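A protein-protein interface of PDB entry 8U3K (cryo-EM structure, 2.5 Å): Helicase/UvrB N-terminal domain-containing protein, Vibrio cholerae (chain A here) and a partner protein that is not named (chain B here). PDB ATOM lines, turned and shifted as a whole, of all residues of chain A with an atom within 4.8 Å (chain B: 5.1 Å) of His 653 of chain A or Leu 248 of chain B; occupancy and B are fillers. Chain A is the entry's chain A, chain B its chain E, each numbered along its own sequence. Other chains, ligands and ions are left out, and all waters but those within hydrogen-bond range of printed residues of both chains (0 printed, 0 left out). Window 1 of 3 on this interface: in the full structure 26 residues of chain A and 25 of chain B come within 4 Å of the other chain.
Among the printed residues, pairs that only touch across the chains: Ser 651 of chain A with Gln 247 of chain B (3.3 Å), Ser 651 of chain A with Leu 248 of chain B (3.9 Å), His 653 of chain A with Ser 242 of chain B (3.6 Å), His 653 of chain A with Ser 244 of chain B (3.3 Å), His 653 of chain A with Leu 248 of chain B (3.7 Å), Phe 654 of chain A with Val 140 of chain B (3.8 Å) and Phe 654 of chain A with Leu 248 of chain B (3.8 Å).
The side-chain hydroxyl (OG) of Ser 651 of chain A lies close to the backbone NH (N) of His 653 of chain A (3.4 Å).
OG of Ser 651 of chain A is in hydrogen-bond range of N of Phe 654 of chain A, 3.2 Å away.
The backbone NH of Ser 244 of chain B lies close to the side-chain hydroxyl of Ser 242 of chain B (3.3 Å).
Of the printed residues of chain B, Arg 650 of chain A touches Gln 247 (2.3 Å).
Of the printed residues of chain B, Ser 651 of chain A touches Ser 244 (3.2 Å), Gln 247 (3.3 Å) and Leu 248 (3.9 Å).
Of the printed residues of chain B, Ser 652 of chain A touches Ser 244.
His 653 of chain A touches just these residues of chain B: Ser 242 (3.6 Å), Ser 244 (3.3 Å) and Leu 248 (3.7 Å).
Of the printed residues of chain B, Phe 654 of chain A touches Val 140 (3.8 Å) and Leu 248 (3.8 Å).
Gln 234 of chain B touches none of the printed residues of chain A.
Of the printed residues of chain A, Ser 244 of chain B touches Ser 651, Ser 652 and His 653.
Of chain A, only Ser 651, His 653 and Phe 654 come within 4 Å of Leu 248 of chain B.
The nearest printed residue of chain B that does not touch Arg 650 of chain A is Leu 248 of chain B (4.04 Å).
The side-chain hydroxyl (OG) of Ser 651 of chain A sits at hydrogen-bond distance from the backbone carbonyl oxygen (O) of Ser 244 of chain B (3.2 Å).
OG of Ser 652 of chain A sits at hydrogen-bond distance from OG of Ser 244 of chain B (3.4 Å).
The guanidinium group (NH1) of Arg 650 of chain A sits close to the backbone carbonyl oxygen (O) of Gln 247 of chain B (2.3 Å).
Of the 11 printed residues of chain B, 5 touch a printed residue of chain A.
Of the 10 printed residues of chain A, 5 touch a printed residue of chain B.
Among the printed residues, no Asp or Glu carboxylate lies within 4 Å of a Lys or Arg side-chain nitrogen of the other chain.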
ATOM      1  N   ARG A 650      13.758 -20.868 -11.565  1.00  0.00           N
ATOM      2  CA  ARG A 650      13.884 -20.075 -10.350  1.00  0.00           C
ATOM      3  C   ARG A 650      15.181 -20.336  -9.600  1.00  0.00           C
ATOM      4  O   ARG A 650      15.996 -19.422  -9.444  1.00  0.00           O
ATOM      5  CB  ARG A 650      12.696 -20.335  -9.425  1.00  0.00           C
ATOM      6  CG  ARG A 650      12.283 -19.119  -8.619  1.00  0.00           C
ATOM      7  CD  ARG A 650      10.923 -19.312  -7.989  1.00  0.00           C
ATOM      8  NE  ARG A 650      10.984 -20.204  -6.839  1.00  0.00           N
ATOM      9  CZ  ARG A 650      10.995 -19.789  -5.579  1.00  0.00           C
ATOM     10  NH1 ARG A 650      11.054 -20.666  -4.593  1.00  0.00           N
ATOM     11  NH2 ARG A 650      10.939 -18.496  -5.305  1.00  0.00           N
ATOM     12  N   SER A 651      15.402 -21.562  -9.140  1.00  0.00           N
ATOM     13  CA  SER A 651      16.560 -21.849  -8.313  1.00  0.00           C
ATOM     14  C   SER A 651      17.276 -23.070  -8.860  1.00  0.00           C
ATOM     15  O   SER A 651      16.661 -23.938  -9.485  1.00  0.00           O
ATOM     16  CB  SER A 651      16.165 -22.086  -6.858  1.00  0.00           C
ATOM     17  OG  SER A 651      16.014 -23.466  -6.607  1.00  0.00           O
ATOM     18  N   SER A 652      18.584 -23.131  -8.610  1.00  0.00           N
ATOM     19  CA  SER A 652      19.393 -24.205  -9.171  1.00  0.00           C
ATOM     20  C   SER A 652      19.055 -25.550  -8.553  1.00  0.00           C
ATOM     21  O   SER A 652      19.197 -26.585  -9.213  1.00  0.00           O
ATOM     22  CB  SER A 652      20.869 -23.899  -8.984  1.00  0.00           C
ATOM     23  OG  SER A 652      21.165 -23.733  -7.616  1.00  0.00           O
ATOM     24  N   HIS A 653      18.622 -25.561  -7.292  1.00  0.00           N
ATOM     25  CA  HIS A 653      18.115 -26.796  -6.706  1.00  0.00           C
ATOM     26  C   HIS A 653      16.909 -27.297  -7.478  1.00  0.00           C
ATOM     27  O   HIS A 653      16.793 -28.494  -7.768  1.00  0.00           O
ATOM     28  CB  HIS A 653      17.747 -26.568  -5.246  1.00  0.00           C
ATOM     29  CG  HIS A 653      18.925 -26.438  -4.337  1.00  0.00           C
ATOM     30  ND1 HIS A 653      19.920 -25.510  -4.539  1.00  0.00           N
ATOM     31  CD2 HIS A 653      19.258 -27.106  -3.209  1.00  0.00           C
ATOM     32  CE1 HIS A 653      20.822 -25.618  -3.582  1.00  0.00           C
ATOM     33  NE2 HIS A 653      20.444 -26.580  -2.762  1.00  0.00           N
ATOM     34  N   PHE A 654      16.013 -26.384  -7.840  1.00  0.00           N
ATOM     35  CA  PHE A 654      14.855 -26.747  -8.638  1.00  0.00           C
ATOM     36  C   PHE A 654      15.262 -27.230 -10.021  1.00  0.00           C
ATOM     37  O   PHE A 654      14.646 -28.150 -10.561  1.00  0.00           O
ATOM     38  CB  PHE A 654      13.905 -25.560  -8.746  1.00  0.00           C
ATOM     39  CG  PHE A 654      12.716 -25.824  -9.602  1.00  0.00           C
ATOM     40  CD1 PHE A 654      11.709 -26.649  -9.161  1.00  0.00           C
ATOM     41  CD2 PHE A 654      12.612 -25.258 -10.852  1.00  0.00           C
ATOM     42  CE1 PHE A 654      10.625 -26.897  -9.945  1.00  0.00           C
ATOM     43  CE2 PHE A 654      11.529 -25.506 -11.639  1.00  0.00           C
ATOM     44  CZ  PHE A 654      10.534 -26.325 -11.187  1.00  0.00           C
ATOM     45  N   ILE A 655      16.281 -26.613 -10.619  1.00  0.00           N
ATOM     46  CA  ILE A 655      16.745 -27.049 -11.933  1.00  0.00           C
ATOM     47  C   ILE A 655      17.291 -28.463 -11.860  1.00  0.00           C
ATOM     48  O   ILE A 655      16.991 -29.307 -12.715  1.00  0.00           O
ATOM     49  CB  ILE A 655      17.789 -26.064 -12.476  1.00  0.00           C
ATOM     50  CG1 ILE A 655      17.132 -24.718 -12.724  1.00  0.00           C
ATOM     51  CG2 ILE A 655      18.399 -26.592 -13.747  1.00  0.00           C
ATOM     52  CD1 ILE A 655      18.070 -23.570 -12.700  1.00  0.00           C
ATOM     53  N   LEU A 656      18.076 -28.748 -10.822  1.00  0.00           N
ATOM     54  CA  LEU A 656      18.574 -30.097 -10.590  1.00  0.00           C
ATOM     55  C   LEU A 656      17.435 -31.089 -10.439  1.00  0.00           C
ATOM     56  O   LEU A 656      17.451 -32.167 -11.043  1.00  0.00           O
ATOM     57  CB  LEU A 656      19.427 -30.114  -9.332  1.00  0.00           C
ATOM     58  CG  LEU A 656      20.878 -30.544  -9.384  1.00  0.00           C
ATOM     59  CD1 LEU A 656      21.312 -30.736  -7.970  1.00  0.00           C
ATOM     60  CD2 LEU A 656      21.026 -31.822 -10.151  1.00  0.00           C
ATOM     61  N   ASN A 657      16.444 -30.749  -9.617  1.00  0.00           N
ATOM     62  CA  ASN A 657      15.347 -31.669  -9.341  1.00  0.00           C
ATOM     63  C   ASN A 657      14.501 -31.910 -10.579  1.00  0.00           C
ATOM     64  O   ASN A 657      14.261 -33.055 -10.976  1.00  0.00           O
ATOM     65  CB  ASN A 657      14.485 -31.107  -8.218  1.00  0.00           C
ATOM     66  CG  ASN A 657      13.475 -32.095  -7.715  1.00  0.00           C
ATOM     67  OD1 ASN A 657      13.444 -33.246  -8.139  1.00  0.00           O
ATOM     68  ND2 ASN A 657      12.626 -31.649  -6.810  1.00  0.00           N
ATOM     69  N   GLN A 667      20.670 -35.539  -4.355  1.00  0.00           N
ATOM     70  CA  GLN A 667      21.097 -34.214  -4.786  1.00  0.00           C
ATOM     71  C   GLN A 667      22.514 -33.911  -4.334  1.00  0.00           C
ATOM     72  O   GLN A 667      23.338 -33.453  -5.127  1.00  0.00           O
ATOM     73  CB  GLN A 667      20.130 -33.156  -4.275  1.00  0.00           C
ATOM     74  CG  GLN A 667      18.859 -33.089  -5.084  1.00  0.00           C
ATOM     75  CD  GLN A 667      18.308 -31.692  -5.180  1.00  0.00           C
ATOM     76  OE1 GLN A 667      18.920 -30.740  -4.701  1.00  0.00           O
ATOM     77  NE2 GLN A 667      17.147 -31.557  -5.803  1.00  0.00           N
ATOM     78  N   ARG A 671      25.615 -33.417  -6.883  1.00  0.00           N
ATOM     79  CA  ARG A 671      26.326 -32.146  -6.854  1.00  0.00           C
ATOM     80  C   ARG A 671      27.799 -32.348  -6.554  1.00  0.00           C
ATOM     81  O   ARG A 671      28.645 -31.590  -7.030  1.00  0.00           O
ATOM     82  CB  ARG A 671      25.709 -31.222  -5.811  1.00  0.00           C
ATOM     83  CG  ARG A 671      24.389 -30.642  -6.219  1.00  0.00           C
ATOM     84  CD  ARG A 671      23.753 -29.857  -5.096  1.00  0.00           C
ATOM     85  NE  ARG A 671      24.424 -28.584  -4.902  1.00  0.00           N
ATOM     86  CZ  ARG A 671      24.161 -27.495  -5.611  1.00  0.00           C
ATOM     87  NH1 ARG A 671      24.821 -26.374  -5.375  1.00  0.00           N
ATOM     88  NH2 ARG A 671      23.235 -27.526  -6.556  1.00  0.00           N
ATOM     89  N   VAL B 140       7.414 -26.453  -5.937  1.00  0.00           N
ATOM     90  CA  VAL B 140       8.615 -26.552  -5.127  1.00  0.00           C
ATOM     91  C   VAL B 140       9.422 -27.797  -5.461  1.00  0.00           C
ATOM     92  O   VAL B 140      10.623 -27.711  -5.723  1.00  0.00           O
ATOM     93  CB  VAL B 140       8.273 -26.517  -3.627  1.00  0.00           C
ATOM     94  CG1 VAL B 140       9.511 -26.712  -2.808  1.00  0.00           C
ATOM     95  CG2 VAL B 140       7.644 -25.205  -3.273  1.00  0.00           C
ATOM     96  N   ILE B 233       6.476 -29.744   2.611  1.00  0.00           N
ATOM     97  CA  ILE B 233       7.570 -28.833   2.327  1.00  0.00           C
ATOM     98  C   ILE B 233       8.085 -28.312   3.656  1.00  0.00           C
ATOM     99  O   ILE B 233       7.296 -27.938   4.529  1.00  0.00           O
ATOM    100  CB  ILE B 233       7.102 -27.682   1.425  1.00  0.00           C
ATOM    101  CG1 ILE B 233       6.551 -28.225   0.117  1.00  0.00           C
ATOM    102  CG2 ILE B 233       8.236 -26.751   1.130  1.00  0.00           C
ATOM    103  CD1 ILE B 233       7.515 -29.098  -0.614  1.00  0.00           C
ATOM    104  N   GLN B 234       9.400 -28.311   3.831  1.00  0.00           N
ATOM    105  CA  GLN B 234       9.972 -27.854   5.086  1.00  0.00           C
ATOM    106  C   GLN B 234       9.750 -26.359   5.261  1.00  0.00           C
ATOM    107  O   GLN B 234       9.550 -25.620   4.299  1.00  0.00           O
ATOM    108  CB  GLN B 234      11.459 -28.179   5.135  1.00  0.00           C
ATOM    109  CG  GLN B 234      12.270 -27.437   4.115  1.00  0.00           C
ATOM    110  CD  GLN B 234      13.196 -28.347   3.356  1.00  0.00           C
ATOM    111  OE1 GLN B 234      13.209 -29.557   3.572  1.00  0.00           O
ATOM    112  NE2 GLN B 234      13.978 -27.773   2.452  1.00  0.00           N
ATOM    113  N   SER B 242      22.488 -21.353   1.707  1.00  0.00           N
ATOM    114  CA  SER B 242      22.208 -21.360   0.283  1.00  0.00           C
ATOM    115  C   SER B 242      20.876 -20.680   0.033  1.00  0.00           C
ATOM    116  O   SER B 242      19.839 -21.144   0.516  1.00  0.00           O
ATOM    117  CB  SER B 242      22.185 -22.789  -0.242  1.00  0.00           C
ATOM    118  OG  SER B 242      21.897 -22.806  -1.626  1.00  0.00           O
ATOM    119  N   SER B 244      19.531 -20.730  -2.761  1.00  0.00           N
ATOM    120  CA  SER B 244      18.830 -21.603  -3.687  1.00  0.00           C
ATOM    121  C   SER B 244      18.035 -22.679  -2.972  1.00  0.00           C
ATOM    122  O   SER B 244      17.121 -23.252  -3.568  1.00  0.00           O
ATOM    123  CB  SER B 244      19.826 -22.234  -4.650  1.00  0.00           C
ATOM    124  OG  SER B 244      20.536 -21.238  -5.358  1.00  0.00           O
ATOM    125  N   GLY B 245      18.366 -22.978  -1.724  1.00  0.00           N
ATOM    126  CA  GLY B 245      17.627 -23.962  -0.962  1.00  0.00           C
ATOM    127  C   GLY B 245      16.624 -23.302  -0.047  1.00  0.00           C
ATOM    128  O   GLY B 245      15.628 -23.906   0.347  1.00  0.00           O
ATOM    129  N   PHE B 246      16.900 -22.050   0.305  1.00  0.00           N
ATOM    130  CA  PHE B 246      15.942 -21.251   1.053  1.00  0.00           C
ATOM    131  C   PHE B 246      14.697 -20.990   0.227  1.00  0.00           C
ATOM    132  O   PHE B 246      13.592 -20.894   0.764  1.00  0.00           O
ATOM    133  CB  PHE B 246      16.602 -19.941   1.469  1.00  0.00           C
ATOM    134  CG  PHE B 246      15.680 -18.962   2.114  1.00  0.00           C
ATOM    135  CD1 PHE B 246      15.429 -19.025   3.460  1.00  0.00           C
ATOM    136  CD2 PHE B 246      15.108 -17.945   1.383  1.00  0.00           C
ATOM    137  CE1 PHE B 246      14.609 -18.119   4.053  1.00  0.00           C
ATOM    138  CE2 PHE B 246      14.284 -17.041   1.979  1.00  0.00           C
ATOM    139  CZ  PHE B 246      14.035 -17.127   3.313  1.00  0.00           C
ATOM    140  N   GLN B 247      14.861 -20.873  -1.088  1.00  0.00           N
ATOM    141  CA  GLN B 247      13.745 -20.576  -1.969  1.00  0.00           C
ATOM    142  C   GLN B 247      12.770 -21.732  -2.088  1.00  0.00           C
ATOM    143  O   GLN B 247      11.631 -21.520  -2.505  1.00  0.00           O
ATOM    144  CB  GLN B 247      14.269 -20.216  -3.350  1.00  0.00           C
ATOM    145  CG  GLN B 247      14.718 -18.800  -3.488  1.00  0.00           C
ATOM    146  CD  GLN B 247      15.364 -18.549  -4.819  1.00  0.00           C
ATOM    147  OE1 GLN B 247      16.284 -19.255  -5.213  1.00  0.00           O
ATOM    148  NE2 GLN B 247      14.881 -17.546  -5.530  1.00  0.00           N
ATOM    149  N   LEU B 248      13.182 -22.942  -1.745  1.00  0.00           N
ATOM    150  CA  LEU B 248      12.328 -24.119  -1.885  1.00  0.00           C
ATOM    151  C   LEU B 248      11.759 -24.547  -0.544  1.00  0.00           C
ATOM    152  O   LEU B 248      11.591 -25.727  -0.263  1.00  0.00           O
ATOM    153  CB  LEU B 248      13.099 -25.256  -2.533  1.00  0.00           C
ATOM    154  CG  LEU B 248      13.680 -25.008  -3.919  1.00  0.00           C
ATOM    155  CD1 LEU B 248      14.157 -26.314  -4.507  1.00  0.00           C
ATOM    156  CD2 LEU B 248      12.657 -24.365  -4.819  1.00  0.00           C
ATOM    157  N   SER B 249      11.464 -23.573   0.306  1.00  0.00           N
ATOM    158  CA  SER B 249      10.856 -23.821   1.598  1.00  0.00           C
ATOM    159  C   SER B 249       9.642 -22.921   1.723  1.00  0.00           C
ATOM    160  O   SER B 249       9.457 -21.998   0.931  1.00  0.00           O
ATOM    161  CB  SER B 249      11.839 -23.568   2.734  1.00  0.00           C
ATOM    162  OG  SER B 249      12.175 -22.202   2.798  1.00  0.00           O
ATOM    163  N   LYS B 250       8.807 -23.203   2.723  1.00  0.00           N
ATOM    164  CA  LYS B 250       7.551 -22.475   2.855  1.00  0.00           C
ATOM    165  C   LYS B 250       7.795 -20.996   3.083  1.00  0.00           C
ATOM    166  O   LYS B 250       7.092 -20.148   2.528  1.00  0.00           O
ATOM    167  CB  LYS B 250       6.722 -23.048   3.992  1.00  0.00           C
ATOM    168  CG  LYS B 250       5.956 -24.281   3.629  1.00  0.00           C
ATOM    169  CD  LYS B 250       5.097 -24.713   4.776  1.00  0.00           C
ATOM    170  CE  LYS B 250       4.276 -25.912   4.417  1.00  0.00           C
ATOM    171  NZ  LYS B 250       3.477 -26.347   5.578  1.00  0.00           N
